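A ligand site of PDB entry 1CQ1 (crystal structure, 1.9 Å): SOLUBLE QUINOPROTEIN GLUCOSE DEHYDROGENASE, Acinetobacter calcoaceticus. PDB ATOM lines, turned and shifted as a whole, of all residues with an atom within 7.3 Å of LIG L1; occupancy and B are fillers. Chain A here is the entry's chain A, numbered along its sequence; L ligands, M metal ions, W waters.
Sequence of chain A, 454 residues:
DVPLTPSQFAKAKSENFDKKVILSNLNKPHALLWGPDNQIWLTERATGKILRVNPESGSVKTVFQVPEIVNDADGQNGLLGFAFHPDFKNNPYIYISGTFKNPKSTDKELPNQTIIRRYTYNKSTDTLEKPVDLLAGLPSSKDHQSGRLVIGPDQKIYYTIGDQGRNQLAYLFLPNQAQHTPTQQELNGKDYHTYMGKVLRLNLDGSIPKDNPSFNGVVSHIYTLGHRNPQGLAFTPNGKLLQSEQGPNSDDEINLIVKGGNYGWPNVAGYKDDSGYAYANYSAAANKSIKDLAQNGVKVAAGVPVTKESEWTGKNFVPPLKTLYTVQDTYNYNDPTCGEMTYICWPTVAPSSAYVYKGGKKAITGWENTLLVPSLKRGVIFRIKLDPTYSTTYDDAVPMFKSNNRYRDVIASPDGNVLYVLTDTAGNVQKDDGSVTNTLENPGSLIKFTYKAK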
ATOM      1  N   ASP A  74      18.233 -26.524  -9.310  1.00  0.00           N
ATOM      2  CA  ASP A  74      19.061 -25.443  -8.775  1.00  0.00           C
ATOM      3  C   ASP A  74      18.223 -24.443  -7.983  1.00  0.00           C
ATOM      4  O   ASP A  74      18.631 -23.287  -7.847  1.00  0.00           O
ATOM      5  CB  ASP A  74      19.757 -24.717  -9.934  1.00  0.00           C
ATOM      6  CG  ASP A  74      18.793 -24.166 -10.965  1.00  0.00           C
ATOM      7  OD1 ASP A  74      17.584 -24.473 -10.915  1.00  0.00           O
ATOM      8  OD2 ASP A  74      19.253 -23.402 -11.848  1.00  0.00           O
ATOM      9  N   GLN A  76      14.941 -23.403  -4.824  1.00  0.00           N
ATOM     10  CA  GLN A  76      14.362 -23.572  -3.498  1.00  0.00           C
ATOM     11  C   GLN A  76      12.849 -23.676  -3.604  1.00  0.00           C
ATOM     12  O   GLN A  76      12.118 -23.496  -2.636  1.00  0.00           O
ATOM     13  CB  GLN A  76      14.760 -22.373  -2.613  1.00  0.00           C
ATOM     14  CG  GLN A  76      16.264 -22.311  -2.362  1.00  0.00           C
ATOM     15  CD  GLN A  76      16.728 -21.000  -1.749  1.00  0.00           C
ATOM     16  OE1 GLN A  76      15.932 -20.149  -1.362  1.00  0.00           O
ATOM     17  NE2 GLN A  76      18.043 -20.823  -1.679  1.00  0.00           N
ATOM     18  N   LYS A 142      12.937 -19.219  -8.120  1.00  0.00           N
ATOM     19  CA  LYS A 142      13.848 -20.252  -7.666  1.00  0.00           C
ATOM     20  C   LYS A 142      14.572 -19.892  -6.374  1.00  0.00           C
ATOM     21  O   LYS A 142      15.353 -20.721  -5.878  1.00  0.00           O
ATOM     22  CB  LYS A 142      14.922 -20.557  -8.714  1.00  0.00           C
ATOM     23  CG  LYS A 142      14.383 -20.989 -10.072  1.00  0.00           C
ATOM     24  CD  LYS A 142      15.544 -21.231 -11.038  1.00  0.00           C
ATOM     25  CE  LYS A 142      15.060 -21.241 -12.472  1.00  0.00           C
ATOM     26  NZ  LYS A 142      16.143 -21.620 -13.421  1.00  0.00           N
ATOM     27  N   ASP A 143      14.325 -18.685  -5.848  1.00  0.00           N
ATOM     28  CA  ASP A 143      15.074 -18.269  -4.656  1.00  0.00           C
ATOM     29  C   ASP A 143      14.178 -17.599  -3.619  1.00  0.00           C
ATOM     30  O   ASP A 143      13.161 -16.978  -3.928  1.00  0.00           O
ATOM     31  CB  ASP A 143      16.188 -17.317  -5.107  1.00  0.00           C
ATOM     32  CG  ASP A 143      17.328 -17.136  -4.128  1.00  0.00           C
ATOM     33  OD1 ASP A 143      17.618 -18.047  -3.321  1.00  0.00           O
ATOM     34  OD2 ASP A 143      17.980 -16.067  -4.136  1.00  0.00           O
ATOM     35  N   HIS A 144      14.617 -17.717  -2.375  1.00  0.00           N
ATOM     36  CA  HIS A 144      13.899 -17.032  -1.279  1.00  0.00           C
ATOM     37  C   HIS A 144      12.395 -17.176  -1.367  1.00  0.00           C
ATOM     38  O   HIS A 144      11.666 -16.201  -1.526  1.00  0.00           O
ATOM     39  CB  HIS A 144      14.252 -15.541  -1.284  1.00  0.00           C
ATOM     40  CG  HIS A 144      15.708 -15.283  -1.032  1.00  0.00           C
ATOM     41  ND1 HIS A 144      16.253 -14.029  -1.183  1.00  0.00           N
ATOM     42  CD2 HIS A 144      16.725 -16.097  -0.648  1.00  0.00           C
ATOM     43  CE1 HIS A 144      17.543 -14.090  -0.903  1.00  0.00           C
ATOM     44  NE2 HIS A 144      17.854 -15.318  -0.572  1.00  0.00           N
ATOM     45  N   GLY A 165      14.313 -13.621  -4.090  1.00  0.00           N
ATOM     46  CA  GLY A 165      15.714 -13.489  -4.426  1.00  0.00           C
ATOM     47  C   GLY A 165      16.048 -12.209  -5.182  1.00  0.00           C
ATOM     48  O   GLY A 165      17.200 -12.017  -5.610  1.00  0.00           O
ATOM     49  N   GLN A 168      19.684  -9.907  -6.119  1.00  0.00           N
ATOM     50  CA  GLN A 168      20.850 -10.749  -5.953  1.00  0.00           C
ATOM     51  C   GLN A 168      20.862 -11.893  -6.991  1.00  0.00           C
ATOM     52  O   GLN A 168      19.812 -12.353  -7.436  1.00  0.00           O
ATOM     53  CB  GLN A 168      21.019 -11.319  -4.556  1.00  0.00           C
ATOM     54  CG  GLN A 168      20.091 -12.445  -4.132  1.00  0.00           C
ATOM     55  CD  GLN A 168      20.720 -13.376  -3.118  1.00  0.00           C
ATOM     56  OE1 GLN A 168      21.753 -13.079  -2.513  1.00  0.00           O
ATOM     57  NE2 GLN A 168      20.118 -14.536  -2.894  1.00  0.00           N
ATOM     58  N   LEU A 169      22.064 -12.360  -7.279  1.00  0.00           N
ATOM     59  CA  LEU A 169      22.265 -13.507  -8.169  1.00  0.00           C
ATOM     60  C   LEU A 169      21.447 -13.417  -9.440  1.00  0.00           C
ATOM     61  O   LEU A 169      21.477 -12.388 -10.123  1.00  0.00           O
ATOM     62  CB  LEU A 169      21.998 -14.788  -7.374  1.00  0.00           C
ATOM     63  CG  LEU A 169      22.894 -15.025  -6.159  1.00  0.00           C
ATOM     64  CD1 LEU A 169      22.319 -16.143  -5.295  1.00  0.00           C
ATOM     65  CD2 LEU A 169      24.317 -15.343  -6.567  1.00  0.00           C
ATOM     66  N   ARG A 228      13.286 -10.777   4.093  1.00  0.00           N
ATOM     67  CA  ARG A 228      14.141 -11.338   3.053  1.00  0.00           C
ATOM     68  C   ARG A 228      13.743 -12.806   2.812  1.00  0.00           C
ATOM     69  O   ARG A 228      12.888 -13.026   1.940  1.00  0.00           O
ATOM     70  CB  ARG A 228      15.605 -11.216   3.420  1.00  0.00           C
ATOM     71  CG  ARG A 228      16.556 -11.632   2.295  1.00  0.00           C
ATOM     72  CD  ARG A 228      17.986 -11.379   2.715  1.00  0.00           C
ATOM     73  NE  ARG A 228      19.020 -11.810   1.798  1.00  0.00           N
ATOM     74  CZ  ARG A 228      19.443 -13.075   1.705  1.00  0.00           C
ATOM     75  NH1 ARG A 228      18.896 -13.998   2.483  1.00  0.00           N
ATOM     76  NH2 ARG A 228      20.411 -13.393   0.837  1.00  0.00           N
ATOM     77  N   ASN A 229      14.246 -13.726   3.617  1.00  0.00           N
ATOM     78  CA  ASN A 229      13.830 -15.125   3.493  1.00  0.00           C
ATOM     79  C   ASN A 229      13.518 -15.761   4.833  1.00  0.00           C
ATOM     80  O   ASN A 229      14.367 -16.437   5.410  1.00  0.00           O
ATOM     81  CB  ASN A 229      14.935 -15.941   2.778  1.00  0.00           C
ATOM     82  CG  ASN A 229      14.501 -17.359   2.444  1.00  0.00           C
ATOM     83  OD1 ASN A 229      13.304 -17.664   2.438  1.00  0.00           O
ATOM     84  ND2 ASN A 229      15.463 -18.228   2.162  1.00  0.00           N
ATOM     85  N   GLN A 246      16.685 -15.451   7.069  1.00  0.00           N
ATOM     86  CA  GLN A 246      17.989 -15.408   6.433  1.00  0.00           C
ATOM     87  C   GLN A 246      18.337 -13.989   5.997  1.00  0.00           C
ATOM     88  O   GLN A 246      17.543 -13.421   5.246  1.00  0.00           O
ATOM     89  CB  GLN A 246      17.957 -16.278   5.149  1.00  0.00           C
ATOM     90  CG  GLN A 246      17.546 -17.720   5.458  1.00  0.00           C
ATOM     91  CD  GLN A 246      18.662 -18.714   5.348  1.00  0.00           C
ATOM     92  OE1 GLN A 246      18.433 -19.940   5.285  1.00  0.00           O
ATOM     93  NE2 GLN A 246      19.894 -18.245   5.310  1.00  0.00           N
ATOM     94  N   GLY A 247      19.503 -13.504   6.415  1.00  0.00           N
ATOM     95  CA  GLY A 247      19.935 -12.174   5.927  1.00  0.00           C
ATOM     96  C   GLY A 247      20.929 -12.429   4.778  1.00  0.00           C
ATOM     97  O   GLY A 247      21.128 -13.588   4.404  1.00  0.00           O
ATOM     98  N   PRO A 248      21.521 -11.388   4.223  1.00  0.00           N
ATOM     99  CA  PRO A 248      22.462 -11.510   3.108  1.00  0.00           C
ATOM    100  C   PRO A 248      23.808 -12.034   3.533  1.00  0.00           C
ATOM    101  O   PRO A 248      23.877 -13.193   3.978  1.00  0.00           O
ATOM    102  CB  PRO A 248      22.489 -10.102   2.539  1.00  0.00           C
ATOM    103  CG  PRO A 248      22.273  -9.236   3.749  1.00  0.00           C
ATOM    104  CD  PRO A 248      21.279  -9.983   4.595  1.00  0.00           C
ATOM    105  N   ASN A 249      24.893 -11.255   3.480  1.00  0.00           N
ATOM    106  CA  ASN A 249      26.186 -11.746   3.940  1.00  0.00           C
ATOM    107  C   ASN A 249      26.276 -11.608   5.463  1.00  0.00           C
ATOM    108  O   ASN A 249      27.234 -12.048   6.103  1.00  0.00           O
ATOM    109  CB  ASN A 249      27.404 -11.046   3.365  1.00  0.00           C
ATOM    110  CG  ASN A 249      27.449 -10.869   1.876  1.00  0.00           C
ATOM    111  OD1 ASN A 249      26.466 -11.072   1.165  1.00  0.00           O
ATOM    112  ND2 ASN A 249      28.634 -10.447   1.416  1.00  0.00           N
ATOM    113  N   ALA A 294      29.346  -8.505  -4.232  1.00  0.00           N
ATOM    114  CA  ALA A 294      29.001  -9.425  -3.145  1.00  0.00           C
ATOM    115  C   ALA A 294      29.705  -9.052  -1.848  1.00  0.00           C
ATOM    116  O   ALA A 294      30.164  -9.905  -1.091  1.00  0.00           O
ATOM    117  CB  ALA A 294      29.357 -10.842  -3.561  1.00  0.00           C
ATOM    118  N   TYR A 343      31.268 -17.527   0.466  1.00  0.00           N
ATOM    119  CA  TYR A 343      30.051 -17.267   1.214  1.00  0.00           C
ATOM    120  C   TYR A 343      29.986 -18.018   2.536  1.00  0.00           C
ATOM    121  O   TYR A 343      29.551 -17.447   3.533  1.00  0.00           O
ATOM    122  CB  TYR A 343      28.802 -17.504   0.371  1.00  0.00           C
ATOM    123  CG  TYR A 343      28.354 -18.925   0.147  1.00  0.00           C
ATOM    124  CD1 TYR A 343      27.455 -19.536   1.024  1.00  0.00           C
ATOM    125  CD2 TYR A 343      28.792 -19.665  -0.945  1.00  0.00           C
ATOM    126  CE1 TYR A 343      27.026 -20.839   0.821  1.00  0.00           C
ATOM    127  CE2 TYR A 343      28.368 -20.961  -1.159  1.00  0.00           C
ATOM    128  CZ  TYR A 343      27.483 -21.547  -0.268  1.00  0.00           C
ATOM    129  OH  TYR A 343      27.061 -22.835  -0.476  1.00  0.00           O
ATOM    130  N   ILE A 344      30.365 -19.288   2.564  1.00  0.00           N
ATOM    131  CA  ILE A 344      30.270 -20.076   3.789  1.00  0.00           C
ATOM    132  C   ILE A 344      30.965 -19.360   4.960  1.00  0.00           C
ATOM    133  O   ILE A 344      30.609 -19.593   6.116  1.00  0.00           O
ATOM    134  CB  ILE A 344      30.865 -21.483   3.578  1.00  0.00           C
ATOM    135  CG1 ILE A 344      29.968 -22.291   2.631  1.00  0.00           C
ATOM    136  CG2 ILE A 344      31.081 -22.223   4.887  1.00  0.00           C
ATOM    137  CD1 ILE A 344      28.652 -22.763   3.226  1.00  0.00           C
ATOM    138  N   TRP A 346      31.062 -16.180   5.386  1.00  0.00           N
ATOM    139  CA  TRP A 346      30.308 -14.970   5.734  1.00  0.00           C
ATOM    140  C   TRP A 346      29.738 -15.119   7.152  1.00  0.00           C
ATOM    141  O   TRP A 346      29.411 -16.226   7.600  1.00  0.00           O
ATOM    142  CB  TRP A 346      29.190 -14.676   4.749  1.00  0.00           C
ATOM    143  CG  TRP A 346      29.533 -14.213   3.364  1.00  0.00           C
ATOM    144  CD1 TRP A 346      30.717 -13.704   2.921  1.00  0.00           C
ATOM    145  CD2 TRP A 346      28.651 -14.209   2.226  1.00  0.00           C
ATOM    146  NE1 TRP A 346      30.632 -13.389   1.582  1.00  0.00           N
ATOM    147  CE2 TRP A 346      29.377 -13.688   1.134  1.00  0.00           C
ATOM    148  CE3 TRP A 346      27.321 -14.603   2.029  1.00  0.00           C
ATOM    149  CZ2 TRP A 346      28.822 -13.536  -0.129  1.00  0.00           C
ATOM    150  CZ3 TRP A 346      26.776 -14.451   0.763  1.00  0.00           C
ATOM    151  CH2 TRP A 346      27.515 -13.923  -0.289  1.00  0.00           C
ATOM    152  N   ARG A 406      23.666 -30.288   6.747  1.00  0.00           N
ATOM    153  CA  ARG A 406      22.892 -29.072   6.610  1.00  0.00           C
ATOM    154  C   ARG A 406      21.551 -29.327   7.307  1.00  0.00           C
ATOM    155  O   ARG A 406      20.705 -30.063   6.800  1.00  0.00           O
ATOM    156  CB  ARG A 406      22.705 -28.676   5.149  1.00  0.00           C
ATOM    157  CG  ARG A 406      23.985 -28.294   4.430  1.00  0.00           C
ATOM    158  CD  ARG A 406      23.754 -28.099   2.947  1.00  0.00           C
ATOM    159  NE  ARG A 406      22.670 -27.207   2.573  1.00  0.00           N
ATOM    160  CZ  ARG A 406      22.756 -25.890   2.459  1.00  0.00           C
ATOM    161  NH1 ARG A 406      23.918 -25.277   2.684  1.00  0.00           N
ATOM    162  NH2 ARG A 406      21.694 -25.201   2.101  1.00  0.00           N
ATOM    163  N   ASN A 428      26.700 -27.321   0.543  1.00  0.00           N
ATOM    164  CA  ASN A 428      27.918 -27.019   1.251  1.00  0.00           C
ATOM    165  C   ASN A 428      27.706 -26.821   2.744  1.00  0.00           C
ATOM    166  O   ASN A 428      26.704 -26.242   3.175  1.00  0.00           O
ATOM    167  CB  ASN A 428      28.538 -25.725   0.683  1.00  0.00           C
ATOM    168  CG  ASN A 428      28.856 -25.842  -0.790  1.00  0.00           C
ATOM    169  OD1 ASN A 428      28.584 -24.926  -1.574  1.00  0.00           O
ATOM    170  ND2 ASN A 428      29.415 -26.986  -1.166  1.00  0.00           N
HETATM  171  C1  LIG L   1      20.934 -17.942  -1.713  1.00  0.00           C
HETATM  172  C2  LIG L   1      21.721 -19.258  -1.716  1.00  0.00           C
HETATM  173  C3  LIG L   1      23.180 -18.848  -1.881  1.00  0.00           C
HETATM  174  C4  LIG L   1      23.648 -18.026  -0.666  1.00  0.00           C
HETATM  175  C5  LIG L   1      24.987 -17.321  -0.830  1.00  0.00           C
HETATM  176  C6  LIG L   1      21.445 -17.074  -0.520  1.00  0.00           C
HETATM  177  O1  LIG L   1      20.807 -15.783  -0.585  1.00  0.00           O
HETATM  178  O2  LIG L   1      19.525 -18.281  -1.606  1.00  0.00           O
HETATM  179  O3  LIG L   1      21.431 -19.966  -2.940  1.00  0.00           O
HETATM  180  O4  LIG L   1      24.000 -19.971  -1.865  1.00  0.00           O
HETATM  181  O5  LIG L   1      22.861 -16.780  -0.652  1.00  0.00           O
HETATM  182  O6  LIG L   1      25.127 -16.549  -1.992  1.00  0.00           O
HETATM  183  N1  LG2 L   2      20.083 -21.638   2.004  1.00  0.00           N
HETATM  184  C1  LG2 L   2      18.757 -21.639   1.729  1.00  0.00           C
HETATM  185  C2  LG2 L   2      18.114 -22.850   1.485  1.00  0.00           C
HETATM  186  O1  LG2 L   2      18.781 -23.877   1.265  1.00  0.00           O
HETATM  187  O2  LG2 L   2      16.906 -22.987   1.456  1.00  0.00           O
HETATM  188  C3  LG2 L   2      18.297 -20.333   1.723  1.00  0.00           C
HETATM  189  C4  LG2 L   2      19.337 -19.520   2.011  1.00  0.00           C
HETATM  190  C5  LG2 L   2      20.439 -20.319   2.184  1.00  0.00           C
HETATM  191  C6  LG2 L   2      19.420 -18.135   2.181  1.00  0.00           C
HETATM  192  O3  LG2 L   2      18.324 -17.296   2.037  1.00  0.00           O
HETATM  193  C7  LG2 L   2      20.607 -17.555   2.531  1.00  0.00           C
HETATM  194  O4  LG2 L   2      20.670 -16.201   2.698  1.00  0.00           O
HETATM  195  C8  LG2 L   2      21.764 -18.353   2.709  1.00  0.00           C
HETATM  196  N2  LG2 L   2      22.827 -17.614   3.076  1.00  0.00           N
HETATM  197  C9  LG2 L   2      23.944 -18.273   3.327  1.00  0.00           C
HETATM  198  C10 LG2 L   2      24.959 -17.413   3.797  1.00  0.00           C
HETATM  199  O5  LG2 L   2      24.719 -16.191   4.009  1.00  0.00           O
HETATM  200  O6  LG2 L   2      26.124 -17.861   4.022  1.00  0.00           O
HETATM  201  C11 LG2 L   2      24.002 -19.639   3.168  1.00  0.00           C
HETATM  202  C12 LG2 L   2      22.895 -20.403   2.759  1.00  0.00           C
HETATM  203  C13 LG2 L   2      23.029 -21.811   2.535  1.00  0.00           C
HETATM  204  O7  LG2 L   2      23.799 -22.524   3.182  1.00  0.00           O
HETATM  205  O8  LG2 L   2      22.392 -22.418   1.682  1.00  0.00           O
HETATM  206  C14 LG2 L   2      21.691 -19.760   2.531  1.00  0.00           C
HETATM  207 CA    CA M   1      22.624 -15.262   3.664  1.00  0.00          CA
HETATM  208  O   HOH W   1      24.286 -14.056  -2.050  1.00  0.00           O
HETATM  209  O   HOH W   2      23.231 -14.798   1.325  1.00  0.00           O
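An oxygen (O2) of LIG L1 is in hydrogen-bond range of the side-chain carboxylate (OD1) of Asp 143 (2.6 Å). NE2 of Gln 168 sits at hydrogen-bond distance from O1 of LIG L1 (2.7 Å). NH2 of Arg 228 is in hydrogen-bond range of O1 of LIG L1, 2.8 Å away. NE2 of Gln 76 is in hydrogen-bond range of O2 of LIG L1 (2.9 Å). A ring nitrogen (NE2) of His 144 is in hydrogen-bond range of an oxygen (O1) of LIG L1. NH1 of Arg 228 lies within hydrogen-bond range of O3 of LG2 L2. An oxygen (O3) of LG2 L2 is in hydrogen-bond range of a ring nitrogen (NE2) of His 144, at 3.3 Å. An oxygen (O3) of LG2 L2 is in hydrogen-bond range of the side-chain amide nitrogen of Asn 229, at 3.0 Å. The side-chain amide nitrogen (NE2) of Gln 246 sits close to an oxygen (O4) of LG2 L2, 3.4 Å away. O7 of LG2 L2 lies within salt-bridge range of NH1 of Arg 406 (2.8 Å).
O1 of LIG L1 sits close to O4 of LG2 L2, at 3.3 Å.
NE2 of Gln 168 sits at hydrogen-bond distance from OD2 of Asp 143. The side-chain amide nitrogen (NE2) of Gln 76 lies within hydrogen-bond range of the side-chain carboxylate (OD1) of Asp 143 (3.3 Å). The side-chain amide nitrogen (NE2) of Gln 168 sits close to a ring nitrogen (NE2) of His 144 (3.3 Å). The guanidinium group of Arg 228 lies close to the backbone carbonyl oxygen of Gly 247. The guanidinium group (NH1) of Arg 228 lies within hydrogen-bond range of the backbone carbonyl oxygen (O) of Gln 246 (3.1 Å). OE1 of Gln 76 is in hydrogen-bond range of N of His 144 (2.9 Å). O of Lys 142 lies within hydrogen-bond range of N of Gln 76, at 2.9 Å. The side-chain amide oxygen of Asn 428 lies within hydrogen-bond range of the side-chain hydroxyl of Tyr 343 (2.8 Å).
Residues that only touch LIG L1: Tyr 343 and Trp 346. Hydrophobic or aromatic side chains that line LIG L1: His 144, Tyr 343 and Trp 346. Within 4 Å of LIG L1: Gln 76, Asp 143, His 144, Gln 168, Arg 228, Tyr 343 and Trp 346. The nearest printed residue that does not touch LIG L1 is Leu 169 (4.2 Å).
Water W1 lies within hydrogen-bond range of O6 of LIG L1 (2.6 Å) and OE1 of Gln 168 (2.8 Å). Water W2 lies within hydrogen-bond range of an oxygen (O5) of LIG L1 (2.8 Å) and the guanidinium group of Arg 228 (3.2 Å).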
